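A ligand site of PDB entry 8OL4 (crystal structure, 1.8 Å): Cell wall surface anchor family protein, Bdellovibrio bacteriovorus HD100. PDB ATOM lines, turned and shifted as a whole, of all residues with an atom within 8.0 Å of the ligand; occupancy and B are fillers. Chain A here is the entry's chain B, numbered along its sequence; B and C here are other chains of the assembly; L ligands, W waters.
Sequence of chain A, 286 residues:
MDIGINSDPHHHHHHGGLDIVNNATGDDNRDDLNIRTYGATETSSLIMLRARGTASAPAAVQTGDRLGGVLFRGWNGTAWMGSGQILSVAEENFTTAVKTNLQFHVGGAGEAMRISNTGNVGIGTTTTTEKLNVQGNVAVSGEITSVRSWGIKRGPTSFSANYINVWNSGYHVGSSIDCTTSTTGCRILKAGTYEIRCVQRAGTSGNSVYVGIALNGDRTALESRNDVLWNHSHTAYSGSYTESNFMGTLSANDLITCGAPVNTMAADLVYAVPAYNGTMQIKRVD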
ATOM      1  N   THR A 118      -4.061 -10.191 -11.002  1.00  0.00           N
ATOM      2  CA  THR A 118      -4.178  -8.885 -10.369  1.00  0.00           C
ATOM      3  C   THR A 118      -3.171  -8.679  -9.260  1.00  0.00           C
ATOM      4  O   THR A 118      -3.119  -7.581  -8.692  1.00  0.00           O
ATOM      5  CB  THR A 118      -5.590  -8.728  -9.772  1.00  0.00           C
ATOM      6  OG1 THR A 118      -5.803  -9.813  -8.880  1.00  0.00           O
ATOM      7  CG2 THR A 118      -6.649  -8.789 -10.866  1.00  0.00           C
ATOM      8  N   ASN A 120      -3.681 -10.310  -6.540  1.00  0.00           N
ATOM      9  CA  ASN A 120      -4.480 -10.626  -5.365  1.00  0.00           C
ATOM     10  C   ASN A 120      -4.223 -12.047  -4.911  1.00  0.00           C
ATOM     11  O   ASN A 120      -4.064 -12.957  -5.735  1.00  0.00           O
ATOM     12  CB  ASN A 120      -5.974 -10.439  -5.641  1.00  0.00           C
ATOM     13  CG  ASN A 120      -6.353  -8.987  -5.846  1.00  0.00           C
ATOM     14  OD1 ASN A 120      -5.508  -8.109  -5.745  1.00  0.00           O
ATOM     15  ND2 ASN A 120      -7.615  -8.732  -6.189  1.00  0.00           N
ATOM     16  N   THR A 128     -10.135 -14.369  -5.571  1.00  0.00           N
ATOM     17  CA  THR A 128      -9.181 -13.363  -5.104  1.00  0.00           C
ATOM     18  C   THR A 128      -9.747 -11.944  -5.293  1.00  0.00           C
ATOM     19  O   THR A 128      -9.181 -11.098  -5.977  1.00  0.00           O
ATOM     20  CB  THR A 128      -7.854 -13.540  -5.822  1.00  0.00           C
ATOM     21  OG1 THR A 128      -8.067 -13.436  -7.236  1.00  0.00           O
ATOM     22  CG2 THR A 128      -7.266 -14.917  -5.500  1.00  0.00           C
ATOM     23  N   THR A 129     -10.883 -11.681  -4.657  1.00  0.00           N
ATOM     24  CA  THR A 129     -11.547 -10.392  -4.822  1.00  0.00           C
ATOM     25  C   THR A 129     -10.676  -9.228  -4.345  1.00  0.00           C
ATOM     26  O   THR A 129     -10.467  -8.257  -5.085  1.00  0.00           O
ATOM     27  CB  THR A 129     -12.881 -10.381  -4.068  1.00  0.00           C
ATOM     28  OG1 THR A 129     -13.741 -11.370  -4.649  1.00  0.00           O
ATOM     29  CG2 THR A 129     -13.527  -9.006  -4.172  1.00  0.00           C
ATOM     30  N   GLU A 130     -10.195  -9.306  -3.106  1.00  0.00           N
ATOM     31  CA  GLU A 130      -9.347  -8.273  -2.520  1.00  0.00           C
ATOM     32  C   GLU A 130      -7.886  -8.685  -2.568  1.00  0.00           C
ATOM     33  O   GLU A 130      -7.528  -9.808  -2.947  1.00  0.00           O
ATOM     34  CB  GLU A 130      -9.761  -7.974  -1.062  1.00  0.00           C
ATOM     35  CG  GLU A 130     -11.258  -7.636  -0.872  1.00  0.00           C
ATOM     36  CD  GLU A 130     -11.673  -6.333  -1.522  1.00  0.00           C
ATOM     37  OE1 GLU A 130     -10.802  -5.503  -1.842  1.00  0.00           O
ATOM     38  OE2 GLU A 130     -12.901  -6.139  -1.714  1.00  0.00           O
ATOM     39  N   LYS A 131      -7.021  -7.752  -2.157  1.00  0.00           N
ATOM     40  CA  LYS A 131      -5.579  -7.998  -2.203  1.00  0.00           C
ATOM     41  C   LYS A 131      -5.219  -9.265  -1.430  1.00  0.00           C
ATOM     42  O   LYS A 131      -4.361 -10.033  -1.872  1.00  0.00           O
ATOM     43  CB  LYS A 131      -4.826  -6.772  -1.676  1.00  0.00           C
ATOM     44  CG  LYS A 131      -3.320  -6.782  -1.959  1.00  0.00           C
ATOM     45  CD  LYS A 131      -2.987  -7.032  -3.447  1.00  0.00           C
ATOM     46  CE  LYS A 131      -3.445  -5.898  -4.356  1.00  0.00           C
ATOM     47  NZ  LYS A 131      -3.231  -6.229  -5.794  1.00  0.00           N
ATOM     48  N   ASN A 133      -7.298 -12.558   0.665  1.00  0.00           N
ATOM     49  CA  ASN A 133      -8.553 -13.222   0.991  1.00  0.00           C
ATOM     50  C   ASN A 133      -8.216 -14.523   1.704  1.00  0.00           C
ATOM     51  O   ASN A 133      -7.401 -15.303   1.213  1.00  0.00           O
ATOM     52  CB  ASN A 133      -9.362 -13.532  -0.277  1.00  0.00           C
ATOM     53  CG  ASN A 133      -9.410 -12.364  -1.243  1.00  0.00           C
ATOM     54  OD1 ASN A 133     -10.399 -11.623  -1.309  1.00  0.00           O
ATOM     55  ND2 ASN A 133      -8.353 -12.199  -2.001  1.00  0.00           N
ATOM     56  N   SER A 175     -14.783   3.721   3.757  1.00  0.00           N
ATOM     57  CA  SER A 175     -15.659   3.549   2.615  1.00  0.00           C
ATOM     58  C   SER A 175     -17.060   3.008   2.934  1.00  0.00           C
ATOM     59  O   SER A 175     -17.871   2.904   2.003  1.00  0.00           O
ATOM     60  CB  SER A 175     -14.980   2.622   1.599  1.00  0.00           C
ATOM     61  OG  SER A 175     -14.797   1.329   2.205  1.00  0.00           O
ATOM     62  N   SER A 176     -17.362   2.664   4.190  1.00  0.00           N
ATOM     63  CA  SER A 176     -18.643   2.031   4.496  1.00  0.00           C
ATOM     64  C   SER A 176     -19.769   3.005   4.862  1.00  0.00           C
ATOM     65  O   SER A 176     -20.929   2.621   4.764  1.00  0.00           O
ATOM     66  CB  SER A 176     -18.481   1.037   5.658  1.00  0.00           C
ATOM     67  OG  SER A 176     -17.642  -0.027   5.294  1.00  0.00           O
ATOM     68  N   LEU A 189     -23.066   2.651   3.015  1.00  0.00           N
ATOM     69  CA  LEU A 189     -22.643   2.385   1.643  1.00  0.00           C
ATOM     70  C   LEU A 189     -22.346   0.906   1.410  1.00  0.00           C
ATOM     71  O   LEU A 189     -22.329   0.471   0.249  1.00  0.00           O
ATOM     72  CB  LEU A 189     -21.396   3.212   1.306  1.00  0.00           C
ATOM     73  CG  LEU A 189     -21.487   4.727   1.570  1.00  0.00           C
ATOM     74  CD1 LEU A 189     -20.141   5.411   1.257  1.00  0.00           C
ATOM     75  CD2 LEU A 189     -22.617   5.358   0.772  1.00  0.00           C
ATOM     76  N   LYS A 190     -22.113   0.147   2.470  1.00  0.00           N
ATOM     77  CA  LYS A 190     -21.738  -1.260   2.360  1.00  0.00           C
ATOM     78  C   LYS A 190     -22.513  -2.068   3.379  1.00  0.00           C
ATOM     79  O   LYS A 190     -22.591  -1.683   4.557  1.00  0.00           O
ATOM     80  CB  LYS A 190     -20.237  -1.437   2.579  1.00  0.00           C
ATOM     81  CG  LYS A 190     -19.372  -0.681   1.567  1.00  0.00           C
ATOM     82  CD  LYS A 190     -17.897  -0.993   1.727  1.00  0.00           C
ATOM     83  CE  LYS A 190     -17.102  -0.452   0.526  1.00  0.00           C
ATOM     84  NZ  LYS A 190     -15.629  -0.709   0.675  1.00  0.00           N
ATOM     85  N   ALA A 191     -23.064  -3.210   2.947  1.00  0.00           N
ATOM     86  CA  ALA A 191     -23.654  -4.139   3.899  1.00  0.00           C
ATOM     87  C   ALA A 191     -22.634  -4.529   4.951  1.00  0.00           C
ATOM     88  O   ALA A 191     -21.470  -4.797   4.636  1.00  0.00           O
ATOM     89  CB  ALA A 191     -24.176  -5.389   3.174  1.00  0.00           C
ATOM     90  N   GLY A 192     -23.054  -4.551   6.214  1.00  0.00           N
ATOM     91  CA  GLY A 192     -22.104  -4.854   7.277  1.00  0.00           C
ATOM     92  C   GLY A 192     -22.770  -4.748   8.623  1.00  0.00           C
ATOM     93  O   GLY A 192     -23.993  -4.580   8.700  1.00  0.00           O
ATOM     94  N   TYR A 194     -22.941  -2.663  12.238  1.00  0.00           N
ATOM     95  CA  TYR A 194     -22.667  -1.322  12.746  1.00  0.00           C
ATOM     96  C   TYR A 194     -23.122  -1.193  14.198  1.00  0.00           C
ATOM     97  O   TYR A 194     -24.116  -1.784  14.617  1.00  0.00           O
ATOM     98  CB  TYR A 194     -23.341  -0.268  11.881  1.00  0.00           C
ATOM     99  CG  TYR A 194     -22.821  -0.319  10.479  1.00  0.00           C
ATOM    100  CD1 TYR A 194     -23.402  -1.188   9.542  1.00  0.00           C
ATOM    101  CD2 TYR A 194     -21.730   0.439  10.083  1.00  0.00           C
ATOM    102  CE1 TYR A 194     -22.911  -1.263   8.249  1.00  0.00           C
ATOM    103  CE2 TYR A 194     -21.254   0.379   8.790  1.00  0.00           C
ATOM    104  CZ  TYR A 194     -21.844  -0.472   7.873  1.00  0.00           C
ATOM    105  OH  TYR A 194     -21.369  -0.548   6.574  1.00  0.00           O
ATOM    106  N   ALA A 252     -26.519  -1.766   2.317  1.00  0.00           N
ATOM    107  CA  ALA A 252     -26.163  -0.666   1.435  1.00  0.00           C
ATOM    108  C   ALA A 252     -27.401   0.130   1.045  1.00  0.00           C
ATOM    109  O   ALA A 252     -28.455  -0.434   0.754  1.00  0.00           O
ATOM    110  CB  ALA A 252     -25.456  -1.193   0.179  1.00  0.00           C
ATOM    111  N   ARG A 284     -18.347   0.851  11.947  1.00  0.00           N
ATOM    112  CA  ARG A 284     -18.433  -0.481  11.375  1.00  0.00           C
ATOM    113  C   ARG A 284     -17.682  -1.460  12.277  1.00  0.00           C
ATOM    114  O   ARG A 284     -16.534  -1.220  12.663  1.00  0.00           O
ATOM    115  CB  ARG A 284     -17.868  -0.528   9.950  1.00  0.00           C
ATOM    116  CG  ARG A 284     -17.829  -1.951   9.437  1.00  0.00           C
ATOM    117  CD  ARG A 284     -18.159  -2.048   7.981  1.00  0.00           C
ATOM    118  NE  ARG A 284     -18.282  -3.442   7.570  1.00  0.00           N
ATOM    119  CZ  ARG A 284     -18.317  -3.837   6.299  1.00  0.00           C
ATOM    120  NH1 ARG A 284     -18.244  -2.931   5.334  1.00  0.00           N
ATOM    121  NH2 ARG A 284     -18.431  -5.115   5.998  1.00  0.00           N
ATOM    122  N   GLY B 136      -3.860  -2.792   0.115  1.00  0.00           N
ATOM    123  CA  GLY B 136      -5.193  -3.099  -0.355  1.00  0.00           C
ATOM    124  C   GLY B 136      -6.051  -3.503   0.824  1.00  0.00           C
ATOM    125  O   GLY B 136      -5.696  -3.262   1.988  1.00  0.00           O
ATOM    126  N   ASN B 137      -7.189  -4.122   0.526  1.00  0.00           N
ATOM    127  CA  ASN B 137      -8.086  -4.613   1.564  1.00  0.00           C
ATOM    128  C   ASN B 137      -7.822  -6.088   1.858  1.00  0.00           C
ATOM    129  O   ASN B 137      -7.197  -6.800   1.065  1.00  0.00           O
ATOM    130  CB  ASN B 137      -9.554  -4.435   1.167  1.00  0.00           C
ATOM    131  CG  ASN B 137      -9.878  -3.024   0.712  1.00  0.00           C
ATOM    132  OD1 ASN B 137      -9.650  -2.057   1.450  1.00  0.00           O
ATOM    133  ND2 ASN B 137     -10.393  -2.895  -0.518  1.00  0.00           N
ATOM    134  N   ALA B 139     -10.073  -9.513   3.086  1.00  0.00           N
ATOM    135  CA  ALA B 139     -11.359 -10.160   3.322  1.00  0.00           C
ATOM    136  C   ALA B 139     -11.121 -11.515   3.999  1.00  0.00           C
ATOM    137  O   ALA B 139     -10.401 -12.361   3.453  1.00  0.00           O
ATOM    138  CB  ALA B 139     -12.126 -10.338   2.014  1.00  0.00           C
ATOM    139  N   GLU C 143      -8.987  -1.640   4.249  1.00  0.00           N
ATOM    140  CA  GLU C 143      -9.882  -2.046   5.321  1.00  0.00           C
ATOM    141  C   GLU C 143      -9.977  -3.569   5.375  1.00  0.00           C
ATOM    142  O   GLU C 143      -9.794  -4.274   4.384  1.00  0.00           O
ATOM    143  CB  GLU C 143     -11.285  -1.445   5.144  1.00  0.00           C
ATOM    144  CG  GLU C 143     -11.281   0.074   5.053  1.00  0.00           C
ATOM    145  CD  GLU C 143     -12.685   0.675   5.057  1.00  0.00           C
ATOM    146  OE1 GLU C 143     -13.552   0.230   5.854  1.00  0.00           O
ATOM    147  OE2 GLU C 143     -12.928   1.593   4.251  1.00  0.00           O
ATOM    148  N   THR C 145     -12.407  -6.748   6.387  1.00  0.00           N
ATOM    149  CA  THR C 145     -13.723  -7.289   6.694  1.00  0.00           C
ATOM    150  C   THR C 145     -13.567  -8.716   7.208  1.00  0.00           C
ATOM    151  O   THR C 145     -12.720  -9.465   6.722  1.00  0.00           O
ATOM    152  CB  THR C 145     -14.632  -7.273   5.447  1.00  0.00           C
ATOM    153  OG1 THR C 145     -14.052  -8.086   4.413  1.00  0.00           O
ATOM    154  CG2 THR C 145     -14.805  -5.847   4.927  1.00  0.00           C
HETATM  155  C1  LIG L   1     -15.184  -4.586  -4.403  1.00  0.00           C
HETATM  156  C2  LIG L   1     -15.957  -5.405  -3.403  1.00  0.00           C
HETATM  157  C3  LIG L   1     -13.994  -5.310  -4.977  1.00  0.00           C
HETATM  158  N1  LIG L   1     -13.165  -4.419  -5.775  1.00  0.00           N
HETATM  159  C4  LIG L   1     -11.823  -4.901  -6.178  1.00  0.00           C
HETATM  160  C5  LIG L   1     -11.157  -3.868  -7.098  1.00  0.00           C
HETATM  161  C6  LIG L   1     -11.930  -6.244  -6.911  1.00  0.00           C
HETATM  162  C7  LIG L   1     -10.952  -5.083  -4.928  1.00  0.00           C
HETATM  163  N2  LIG L   1     -17.012  -4.605  -2.765  1.00  0.00           N
HETATM  164  C8  LIG L   1     -17.544  -5.072  -1.462  1.00  0.00           C
HETATM  165  C9  LIG L   1     -18.683  -4.128  -1.064  1.00  0.00           C
HETATM  166  C10 LIG L   1     -16.448  -5.029  -0.395  1.00  0.00           C
HETATM  167  C11 LIG L   1     -18.064  -6.502  -1.577  1.00  0.00           C
HETATM  168  O1  LIG L   1     -19.117  -4.354   0.267  1.00  0.00           O
HETATM  169  O2  LIG L   1     -15.997  -3.703  -0.176  1.00  0.00           O
HETATM  170  O3  LIG L   1     -18.890  -6.665  -2.723  1.00  0.00           O
HETATM  171  O4  LIG L   1     -12.073  -3.353  -8.047  1.00  0.00           O
HETATM  172  O5  LIG L   1     -12.796  -6.150  -8.027  1.00  0.00           O
HETATM  173  O6  LIG L   1     -10.987  -3.918  -4.118  1.00  0.00           O
HETATM  174  O   HOH W   1     -14.499  -7.885  -0.598  1.00  0.00           O
HETATM  175  O   HOH W   2     -17.859  -4.707   3.140  1.00  0.00           O
HETATM  176  O   HOH W   3     -22.586  -3.903   0.232  1.00  0.00           O
HETATM  177  O   HOH W   4     -10.319  -9.008  -8.310  1.00  0.00           O
HETATM  178  O   HOH W   5     -15.193  -3.051   2.757  1.00  0.00           O
HETATM  179  O   HOH W   6     -13.402  -3.490  -1.398  1.00  0.00           O
HETATM  180  O   HOH W   7     -17.885  -9.060  -4.353  1.00  0.00           O
HETATM  181  O   HOH W   8     -21.090  -6.562   0.239  1.00  0.00           O
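OE1 of Glu 130 lies within hydrogen-bond range of O6 of the ligand (2.8 Å). NZ of Lys 190 lies within hydrogen-bond range of O2 of the ligand, 3.1 Å away.
Residues that only touch the ligand: Thr 129 (3.1 Å) and Asn 137 of chain B (3.8 Å). Four residues have an atom within 4 Å of the ligand: Thr 129, Glu 130, Lys 190 and Asn 137 of chain B. The nearest printed residue that does not touch the ligand is Ala 191 (4.9 Å).
Water W6 lies within hydrogen-bond range of the side-chain carboxylate (OE2) of Glu 130 (2.7 Å), an oxygen (O2) of the ligand (2.9 Å) and the side-chain amide nitrogen (ND2) of Asn 137 of chain B (3.2 Å). Water W5 bridges an oxygen (O2) of the ligand (3.1 Å) and the side-chain amino group (NZ) of Lys 190 (3.2 Å). Water W2 bridges the guanidinium group (NH1) of Arg 284 (2.8 Å) and an oxygen (O1) of the ligand (3.2 Å). Water W4 lies within hydrogen-bond range of the backbone carbonyl oxygen (O) of Thr 129 (3.3 Å), the backbone carbonyl oxygen (O) of Thr 128 (3.3 Å) and the side-chain amide nitrogen (ND2) of Asn 120 (3.4 Å). Water W3 lies within hydrogen-bond range of N of Ala 191 (2.8 Å) and O1 of the ligand (3.5 Å).
O of Glu 130 lies close to ND2 of Asn 120, at 3.4 Å. The side-chain hydroxyl of Tyr 194 sits at hydrogen-bond distance from the backbone carbonyl oxygen of Lys 190, at 2.6 Å. The side-chain carboxylate of Glu 130 is in hydrogen-bond range of the side-chain amide nitrogen of Asn 137 of chain B (3.0 Å). N of Thr 129 is in hydrogen-bond range of OD1 of Asn 133 (3.4 Å). The backbone carbonyl oxygen (O) of Asn 137 of chain B is in hydrogen-bond range of the backbone NH (N) of Lys 131, 3.4 Å away. O of Thr 129 lies within hydrogen-bond range of ND2 of Asn 120 (3.1 Å). ND2 of Asn 133 is in hydrogen-bond range of O of Glu 130, 2.7 Å away. N of Glu 143 of chain C sits at hydrogen-bond distance from OD1 of Asn 137 of chain B, at 2.9 Å.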
